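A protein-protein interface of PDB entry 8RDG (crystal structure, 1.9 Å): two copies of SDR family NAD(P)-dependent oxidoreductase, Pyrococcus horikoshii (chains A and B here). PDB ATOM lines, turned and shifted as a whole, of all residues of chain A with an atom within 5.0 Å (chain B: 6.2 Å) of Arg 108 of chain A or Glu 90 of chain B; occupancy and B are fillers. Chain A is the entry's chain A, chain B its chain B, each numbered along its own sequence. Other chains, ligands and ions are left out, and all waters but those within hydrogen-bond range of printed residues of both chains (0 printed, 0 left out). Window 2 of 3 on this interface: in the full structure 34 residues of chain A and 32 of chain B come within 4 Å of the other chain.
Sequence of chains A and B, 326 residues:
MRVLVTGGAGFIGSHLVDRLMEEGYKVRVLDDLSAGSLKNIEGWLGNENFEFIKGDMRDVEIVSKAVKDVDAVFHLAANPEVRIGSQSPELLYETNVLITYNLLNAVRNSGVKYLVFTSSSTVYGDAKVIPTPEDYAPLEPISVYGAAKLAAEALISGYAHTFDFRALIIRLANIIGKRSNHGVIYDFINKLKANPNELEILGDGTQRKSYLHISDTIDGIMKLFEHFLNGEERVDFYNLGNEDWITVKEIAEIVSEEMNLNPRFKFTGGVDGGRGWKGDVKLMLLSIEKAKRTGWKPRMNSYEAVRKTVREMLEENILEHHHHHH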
ATOM      1  N   TYR A 101      11.379  20.985  26.145  1.00  0.00           N
ATOM      2  CA  TYR A 101      11.382  19.554  25.854  1.00  0.00           C
ATOM      3  C   TYR A 101      12.389  19.219  24.755  1.00  0.00           C
ATOM      4  O   TYR A 101      13.178  18.273  24.892  1.00  0.00           O
ATOM      5  CB  TYR A 101       9.967  19.131  25.458  1.00  0.00           C
ATOM      6  CG  TYR A 101       9.815  17.776  24.775  1.00  0.00           C
ATOM      7  CD1 TYR A 101      10.026  16.589  25.462  1.00  0.00           C
ATOM      8  CD2 TYR A 101       9.408  17.700  23.443  1.00  0.00           C
ATOM      9  CE1 TYR A 101       9.861  15.359  24.839  1.00  0.00           C
ATOM     10  CE2 TYR A 101       9.226  16.481  22.811  1.00  0.00           C
ATOM     11  CZ  TYR A 101       9.452  15.317  23.516  1.00  0.00           C
ATOM     12  OH  TYR A 101       9.284  14.114  22.889  1.00  0.00           O
ATOM     13  N   LEU A 104      15.851  19.424  26.098  1.00  0.00           N
ATOM     14  CA  LEU A 104      16.173  18.309  26.973  1.00  0.00           C
ATOM     15  C   LEU A 104      16.464  17.045  26.166  1.00  0.00           C
ATOM     16  O   LEU A 104      17.362  16.270  26.520  1.00  0.00           O
ATOM     17  CB  LEU A 104      15.039  18.092  27.975  1.00  0.00           C
ATOM     18  CG  LEU A 104      14.895  19.172  29.056  1.00  0.00           C
ATOM     19  CD1 LEU A 104      13.540  19.074  29.771  1.00  0.00           C
ATOM     20  CD2 LEU A 104      16.042  19.093  30.059  1.00  0.00           C
ATOM     21  N   ASN A 105      15.723  16.821  25.073  1.00  0.00           N
ATOM     22  CA  ASN A 105      16.031  15.677  24.215  1.00  0.00           C
ATOM     23  C   ASN A 105      17.404  15.837  23.569  1.00  0.00           C
ATOM     24  O   ASN A 105      18.147  14.857  23.414  1.00  0.00           O
ATOM     25  CB  ASN A 105      14.958  15.502  23.147  1.00  0.00           C
ATOM     26  CG  ASN A 105      13.706  14.881  23.697  1.00  0.00           C
ATOM     27  OD1 ASN A 105      13.764  14.123  24.659  1.00  0.00           O
ATOM     28  ND2 ASN A 105      12.569  15.185  23.086  1.00  0.00           N
ATOM     29  N   ALA A 106      17.773  17.074  23.231  1.00  0.00           N
ATOM     30  CA  ALA A 106      19.100  17.323  22.676  1.00  0.00           C
ATOM     31  C   ALA A 106      20.209  17.118  23.708  1.00  0.00           C
ATOM     32  O   ALA A 106      21.316  16.696  23.359  1.00  0.00           O
ATOM     33  CB  ALA A 106      19.165  18.736  22.115  1.00  0.00           C
ATOM     34  N   VAL A 107      19.950  17.475  24.968  1.00  0.00           N
ATOM     35  CA  VAL A 107      20.961  17.424  26.019  1.00  0.00           C
ATOM     36  C   VAL A 107      21.301  15.984  26.362  1.00  0.00           C
ATOM     37  O   VAL A 107      22.440  15.669  26.732  1.00  0.00           O
ATOM     38  CB  VAL A 107      20.468  18.217  27.244  1.00  0.00           C
ATOM     39  CG1 VAL A 107      21.187  17.769  28.513  1.00  0.00           C
ATOM     40  CG2 VAL A 107      20.646  19.703  27.008  1.00  0.00           C
ATOM     41  N   ARG A 108      20.337  15.088  26.210  1.00  0.00           N
ATOM     42  CA  ARG A 108      20.531  13.684  26.526  1.00  0.00           C
ATOM     43  C   ARG A 108      21.707  13.113  25.723  1.00  0.00           C
ATOM     44  O   ARG A 108      21.737  13.208  24.492  1.00  0.00           O
ATOM     45  CB  ARG A 108      19.230  12.945  26.221  1.00  0.00           C
ATOM     46  CG  ARG A 108      19.385  11.502  25.927  1.00  0.00           C
ATOM     47  CD  ARG A 108      18.028  10.799  25.878  1.00  0.00           C
ATOM     48  NE  ARG A 108      17.074  11.436  24.971  1.00  0.00           N
ATOM     49  CZ  ARG A 108      16.074  10.791  24.378  1.00  0.00           C
ATOM     50  NH1 ARG A 108      15.872   9.496  24.583  1.00  0.00           N
ATOM     51  NH2 ARG A 108      15.265  11.459  23.557  1.00  0.00           N
ATOM     52  N   ASN A 109      22.699  12.573  26.445  1.00  0.00           N
ATOM     53  CA  ASN A 109      23.903  11.946  25.875  1.00  0.00           C
ATOM     54  C   ASN A 109      24.779  12.930  25.102  1.00  0.00           C
ATOM     55  O   ASN A 109      25.558  12.530  24.235  1.00  0.00           O
ATOM     56  CB  ASN A 109      23.541  10.780  24.955  1.00  0.00           C
ATOM     57  CG  ASN A 109      23.010   9.591  25.706  1.00  0.00           C
ATOM     58  OD1 ASN A 109      23.467   9.274  26.807  1.00  0.00           O
ATOM     59  ND2 ASN A 109      22.042   8.917  25.111  1.00  0.00           N
ATOM     60  N   SER A 110      24.742  14.207  25.450  1.00  0.00           N
ATOM     61  CA  SER A 110      25.488  15.199  24.691  1.00  0.00           C
ATOM     62  C   SER A 110      26.730  15.647  25.416  1.00  0.00           C
ATOM     63  O   SER A 110      27.529  16.399  24.848  1.00  0.00           O
ATOM     64  CB  SER A 110      24.636  16.450  24.444  1.00  0.00           C
ATOM     65  OG  SER A 110      24.483  17.168  25.679  1.00  0.00           O
ATOM     66  N   TYR A 159      14.516  14.826  33.411  1.00  0.00           N
ATOM     67  CA  TYR A 159      15.616  14.514  32.500  1.00  0.00           C
ATOM     68  C   TYR A 159      16.964  14.552  33.210  1.00  0.00           C
ATOM     69  O   TYR A 159      17.837  13.724  32.934  1.00  0.00           O
ATOM     70  CB  TYR A 159      15.631  15.484  31.328  1.00  0.00           C
ATOM     71  CG  TYR A 159      14.745  15.105  30.183  1.00  0.00           C
ATOM     72  CD1 TYR A 159      13.359  15.181  30.296  1.00  0.00           C
ATOM     73  CD2 TYR A 159      15.284  14.686  28.978  1.00  0.00           C
ATOM     74  CE1 TYR A 159      12.534  14.855  29.231  1.00  0.00           C
ATOM     75  CE2 TYR A 159      14.468  14.361  27.905  1.00  0.00           C
ATOM     76  CZ  TYR A 159      13.094  14.444  28.040  1.00  0.00           C
ATOM     77  OH  TYR A 159      12.280  14.114  26.973  1.00  0.00           O
ATOM     78  N   PHE A 163      19.070  11.179  32.810  1.00  0.00           N
ATOM     79  CA  PHE A 163      20.177  11.163  31.863  1.00  0.00           C
ATOM     80  C   PHE A 163      21.430  11.799  32.441  1.00  0.00           C
ATOM     81  O   PHE A 163      22.361  12.124  31.699  1.00  0.00           O
ATOM     82  CB  PHE A 163      19.754  11.831  30.553  1.00  0.00           C
ATOM     83  CG  PHE A 163      18.551  11.185  29.939  1.00  0.00           C
ATOM     84  CD1 PHE A 163      18.624   9.893  29.441  1.00  0.00           C
ATOM     85  CD2 PHE A 163      17.339  11.854  29.872  1.00  0.00           C
ATOM     86  CE1 PHE A 163      17.515   9.275  28.888  1.00  0.00           C
ATOM     87  CE2 PHE A 163      16.232  11.249  29.316  1.00  0.00           C
ATOM     88  CZ  PHE A 163      16.318   9.951  28.825  1.00  0.00           C
ATOM     89  N   ARG B  58      -4.099  12.752  20.511  1.00  0.00           N
ATOM     90  CA  ARG B  58      -3.215  13.578  19.688  1.00  0.00           C
ATOM     91  C   ARG B  58      -3.981  14.296  18.588  1.00  0.00           C
ATOM     92  O   ARG B  58      -3.454  15.244  18.001  1.00  0.00           O
ATOM     93  CB  ARG B  58      -2.125  12.724  19.053  1.00  0.00           C
ATOM     94  CG  ARG B  58      -1.175  12.045  20.022  1.00  0.00           C
ATOM     95  CD  ARG B  58      -0.398  10.970  19.256  1.00  0.00           C
ATOM     96  NE  ARG B  58       0.611  10.328  20.087  1.00  0.00           N
ATOM     97  CZ  ARG B  58       0.395   9.252  20.829  1.00  0.00           C
ATOM     98  NH1 ARG B  58      -0.802   8.681  20.896  1.00  0.00           N
ATOM     99  NH2 ARG B  58       1.407   8.723  21.511  1.00  0.00           N
ATOM    100  N   SER B  88       9.977   5.408  26.139  1.00  0.00           N
ATOM    101  CA  SER B  88      10.863   6.463  25.674  1.00  0.00           C
ATOM    102  C   SER B  88      10.354   7.821  26.126  1.00  0.00           C
ATOM    103  O   SER B  88       9.163   7.991  26.390  1.00  0.00           O
ATOM    104  CB  SER B  88      10.958   6.438  24.158  1.00  0.00           C
ATOM    105  OG  SER B  88       9.844   7.093  23.574  1.00  0.00           O
ATOM    106  N   PRO B  89      11.238   8.813  26.226  1.00  0.00           N
ATOM    107  CA  PRO B  89      10.765  10.140  26.641  1.00  0.00           C
ATOM    108  C   PRO B  89       9.734  10.718  25.691  1.00  0.00           C
ATOM    109  O   PRO B  89       8.794  11.381  26.132  1.00  0.00           O
ATOM    110  CB  PRO B  89      12.048  10.983  26.662  1.00  0.00           C
ATOM    111  CG  PRO B  89      13.164  10.006  26.748  1.00  0.00           C
ATOM    112  CD  PRO B  89      12.701   8.760  26.065  1.00  0.00           C
ATOM    113  N   GLU B  90       9.875  10.471  24.392  1.00  0.00           N
ATOM    114  CA  GLU B  90       8.928  11.022  23.433  1.00  0.00           C
ATOM    115  C   GLU B  90       7.527  10.478  23.675  1.00  0.00           C
ATOM    116  O   GLU B  90       6.544  11.230  23.646  1.00  0.00           O
ATOM    117  CB  GLU B  90       9.403  10.729  22.007  1.00  0.00           C
ATOM    118  CG  GLU B  90      10.743  11.402  21.645  1.00  0.00           C
ATOM    119  CD  GLU B  90      11.961  10.597  22.080  1.00  0.00           C
ATOM    120  OE1 GLU B  90      11.787   9.466  22.591  1.00  0.00           O
ATOM    121  OE2 GLU B  90      13.102  11.097  21.918  1.00  0.00           O
ATOM    122  N   LEU B  91       7.417   9.171  23.921  1.00  0.00           N
ATOM    123  CA  LEU B  91       6.107   8.594  24.193  1.00  0.00           C
ATOM    124  C   LEU B  91       5.510   9.192  25.460  1.00  0.00           C
ATOM    125  O   LEU B  91       4.312   9.502  25.508  1.00  0.00           O
ATOM    126  CB  LEU B  91       6.220   7.070  24.305  1.00  0.00           C
ATOM    127  CG  LEU B  91       4.998   6.308  24.806  1.00  0.00           C
ATOM    128  CD1 LEU B  91       3.828   6.570  23.886  1.00  0.00           C
ATOM    129  CD2 LEU B  91       5.315   4.826  24.836  1.00  0.00           C
ATOM    130  N   LEU B  92       6.332   9.354  26.497  1.00  0.00           N
ATOM    131  CA  LEU B  92       5.828   9.888  27.755  1.00  0.00           C
ATOM    132  C   LEU B  92       5.381  11.330  27.598  1.00  0.00           C
ATOM    133  O   LEU B  92       4.321  11.715  28.111  1.00  0.00           O
ATOM    134  CB  LEU B  92       6.892   9.767  28.843  1.00  0.00           C
ATOM    135  CG  LEU B  92       7.306   8.354  29.233  1.00  0.00           C
ATOM    136  CD1 LEU B  92       8.405   8.411  30.284  1.00  0.00           C
ATOM    137  CD2 LEU B  92       6.114   7.632  29.766  1.00  0.00           C
ATOM    138  N   TYR B  93       6.155  12.137  26.873  1.00  0.00           N
ATOM    139  CA  TYR B  93       5.754  13.521  26.641  1.00  0.00           C
ATOM    140  C   TYR B  93       4.439  13.567  25.873  1.00  0.00           C
ATOM    141  O   TYR B  93       3.509  14.262  26.274  1.00  0.00           O
ATOM    142  CB  TYR B  93       6.850  14.291  25.899  1.00  0.00           C
ATOM    143  CG  TYR B  93       6.496  15.733  25.585  1.00  0.00           C
ATOM    144  CD1 TYR B  93       6.753  16.736  26.518  1.00  0.00           C
ATOM    145  CD2 TYR B  93       5.901  16.094  24.381  1.00  0.00           C
ATOM    146  CE1 TYR B  93       6.442  18.057  26.254  1.00  0.00           C
ATOM    147  CE2 TYR B  93       5.579  17.424  24.110  1.00  0.00           C
ATOM    148  CZ  TYR B  93       5.853  18.397  25.055  1.00  0.00           C
ATOM    149  OH  TYR B  93       5.551  19.730  24.817  1.00  0.00           O
ATOM    150  N   GLU B  94       4.321  12.782  24.801  1.00  0.00           N
ATOM    151  CA  GLU B  94       3.111  12.830  23.987  1.00  0.00           C
ATOM    152  C   GLU B  94       1.885  12.381  24.772  1.00  0.00           C
ATOM    153  O   GLU B  94       0.840  13.034  24.710  1.00  0.00           O
ATOM    154  CB  GLU B  94       3.280  11.969  22.746  1.00  0.00           C
ATOM    155  CG  GLU B  94       4.187  12.613  21.707  1.00  0.00           C
ATOM    156  CD  GLU B  94       4.605  11.633  20.636  1.00  0.00           C
ATOM    157  OE1 GLU B  94       3.875  10.629  20.440  1.00  0.00           O
ATOM    158  OE2 GLU B  94       5.664  11.863  20.004  1.00  0.00           O
ATOM    159  N   THR B  95       1.989  11.285  25.530  1.00  0.00           N
ATOM    160  CA  THR B  95       0.827  10.745  26.231  1.00  0.00           C
ATOM    161  C   THR B  95       0.572  11.387  27.588  1.00  0.00           C
ATOM    162  O   THR B  95      -0.399  11.006  28.258  1.00  0.00           O
ATOM    163  CB  THR B  95       0.966   9.233  26.429  1.00  0.00           C
ATOM    164  OG1 THR B  95       2.199   8.965  27.110  1.00  0.00           O
ATOM    165  CG2 THR B  95       0.944   8.522  25.084  1.00  0.00           C
ATOM    166  N   VAL B 144      11.217  10.570  33.772  1.00  0.00           N
ATOM    167  CA  VAL B 144      10.493  11.340  32.769  1.00  0.00           C
ATOM    168  C   VAL B 144       8.990  11.172  32.954  1.00  0.00           C
ATOM    169  O   VAL B 144       8.225  12.111  32.721  1.00  0.00           O
ATOM    170  CB  VAL B 144      10.943  10.942  31.351  1.00  0.00           C
ATOM    171  CG1 VAL B 144      10.086  11.654  30.304  1.00  0.00           C
ATOM    172  CG2 VAL B 144      12.413  11.254  31.148  1.00  0.00           C
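The side-chain amide nitrogen (ND2) of Asn 105 of chain A sits close to the side-chain hydroxyl (OH) of Tyr 101 of chain A (3.5 Å).
OD1 of Asn 105 of chain A is in hydrogen-bond range of NH2 of Arg 108 of chain A, 3.3 Å away.
The side-chain hydroxyl of Tyr 159 of chain A is in hydrogen-bond range of the side-chain amide oxygen of Asn 105 of chain A (2.7 Å).
OG of Ser 88 of chain B lies within hydrogen-bond range of OE1 of Glu 90 of chain B (3.2 Å).
Of the printed residues of chain B, Arg 108 of chain A touches Pro 89 and Glu 90.
Of chain A, only Tyr 101 and Arg 108 come within 4 Å of Glu 90 of chain B.
Printed residues of chain A within 4 Å of Tyr 93 of chain B: Tyr 101.
Of the printed residues of chain A, Pro 89 of chain B touches Arg 108 (3.5 Å), Tyr 159 (3.2 Å) and Phe 163 (3.8 Å).
Of the printed residues of chain B, Tyr 159 of chain A touches Pro 89 (3.2 Å).
Printed residues of chain B within 4 Å of Phe 163 of chain A: Pro 89.
Printed residues of chain B within 4 Å of Tyr 101 of chain A: Glu 90 (3.2 Å) and Tyr 93 (3.4 Å).
The nearest printed residue of chain A that does not touch Tyr 93 of chain B is Tyr 159 of chain A (5.5 Å).
Among the printed residues, merely in contact across the chains: Tyr 159 of chain A with Pro 89 of chain B, Tyr 101 of chain A with Glu 90 of chain B, Tyr 101 of chain A with Tyr 93 of chain B, Arg 108 of chain A with Pro 89 of chain B and Phe 163 of chain A with Pro 89 of chain B.
The guanidinium group of Arg 108 of chain A lies within salt-bridge range of the side-chain carboxylate of Glu 90 of chain B.
No position is printed for both chains.
Of the 6 pairs that touch across the chains among the printed residues, none has its exchanged pair printed and touching as well.
Printed residues of chain A that touch a printed residue of chain B: Tyr 101, Arg 108, Tyr 159 and Phe 163.
Hydrophobic or aromatic side chains of chain A that line the printed part of chain B: Tyr 101, Tyr 159 and Phe 163.
Of the 10 printed residues of chain B, 3 touch a printed residue of chain A.
Among the printed residues, 6 pairs touch across the chains.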
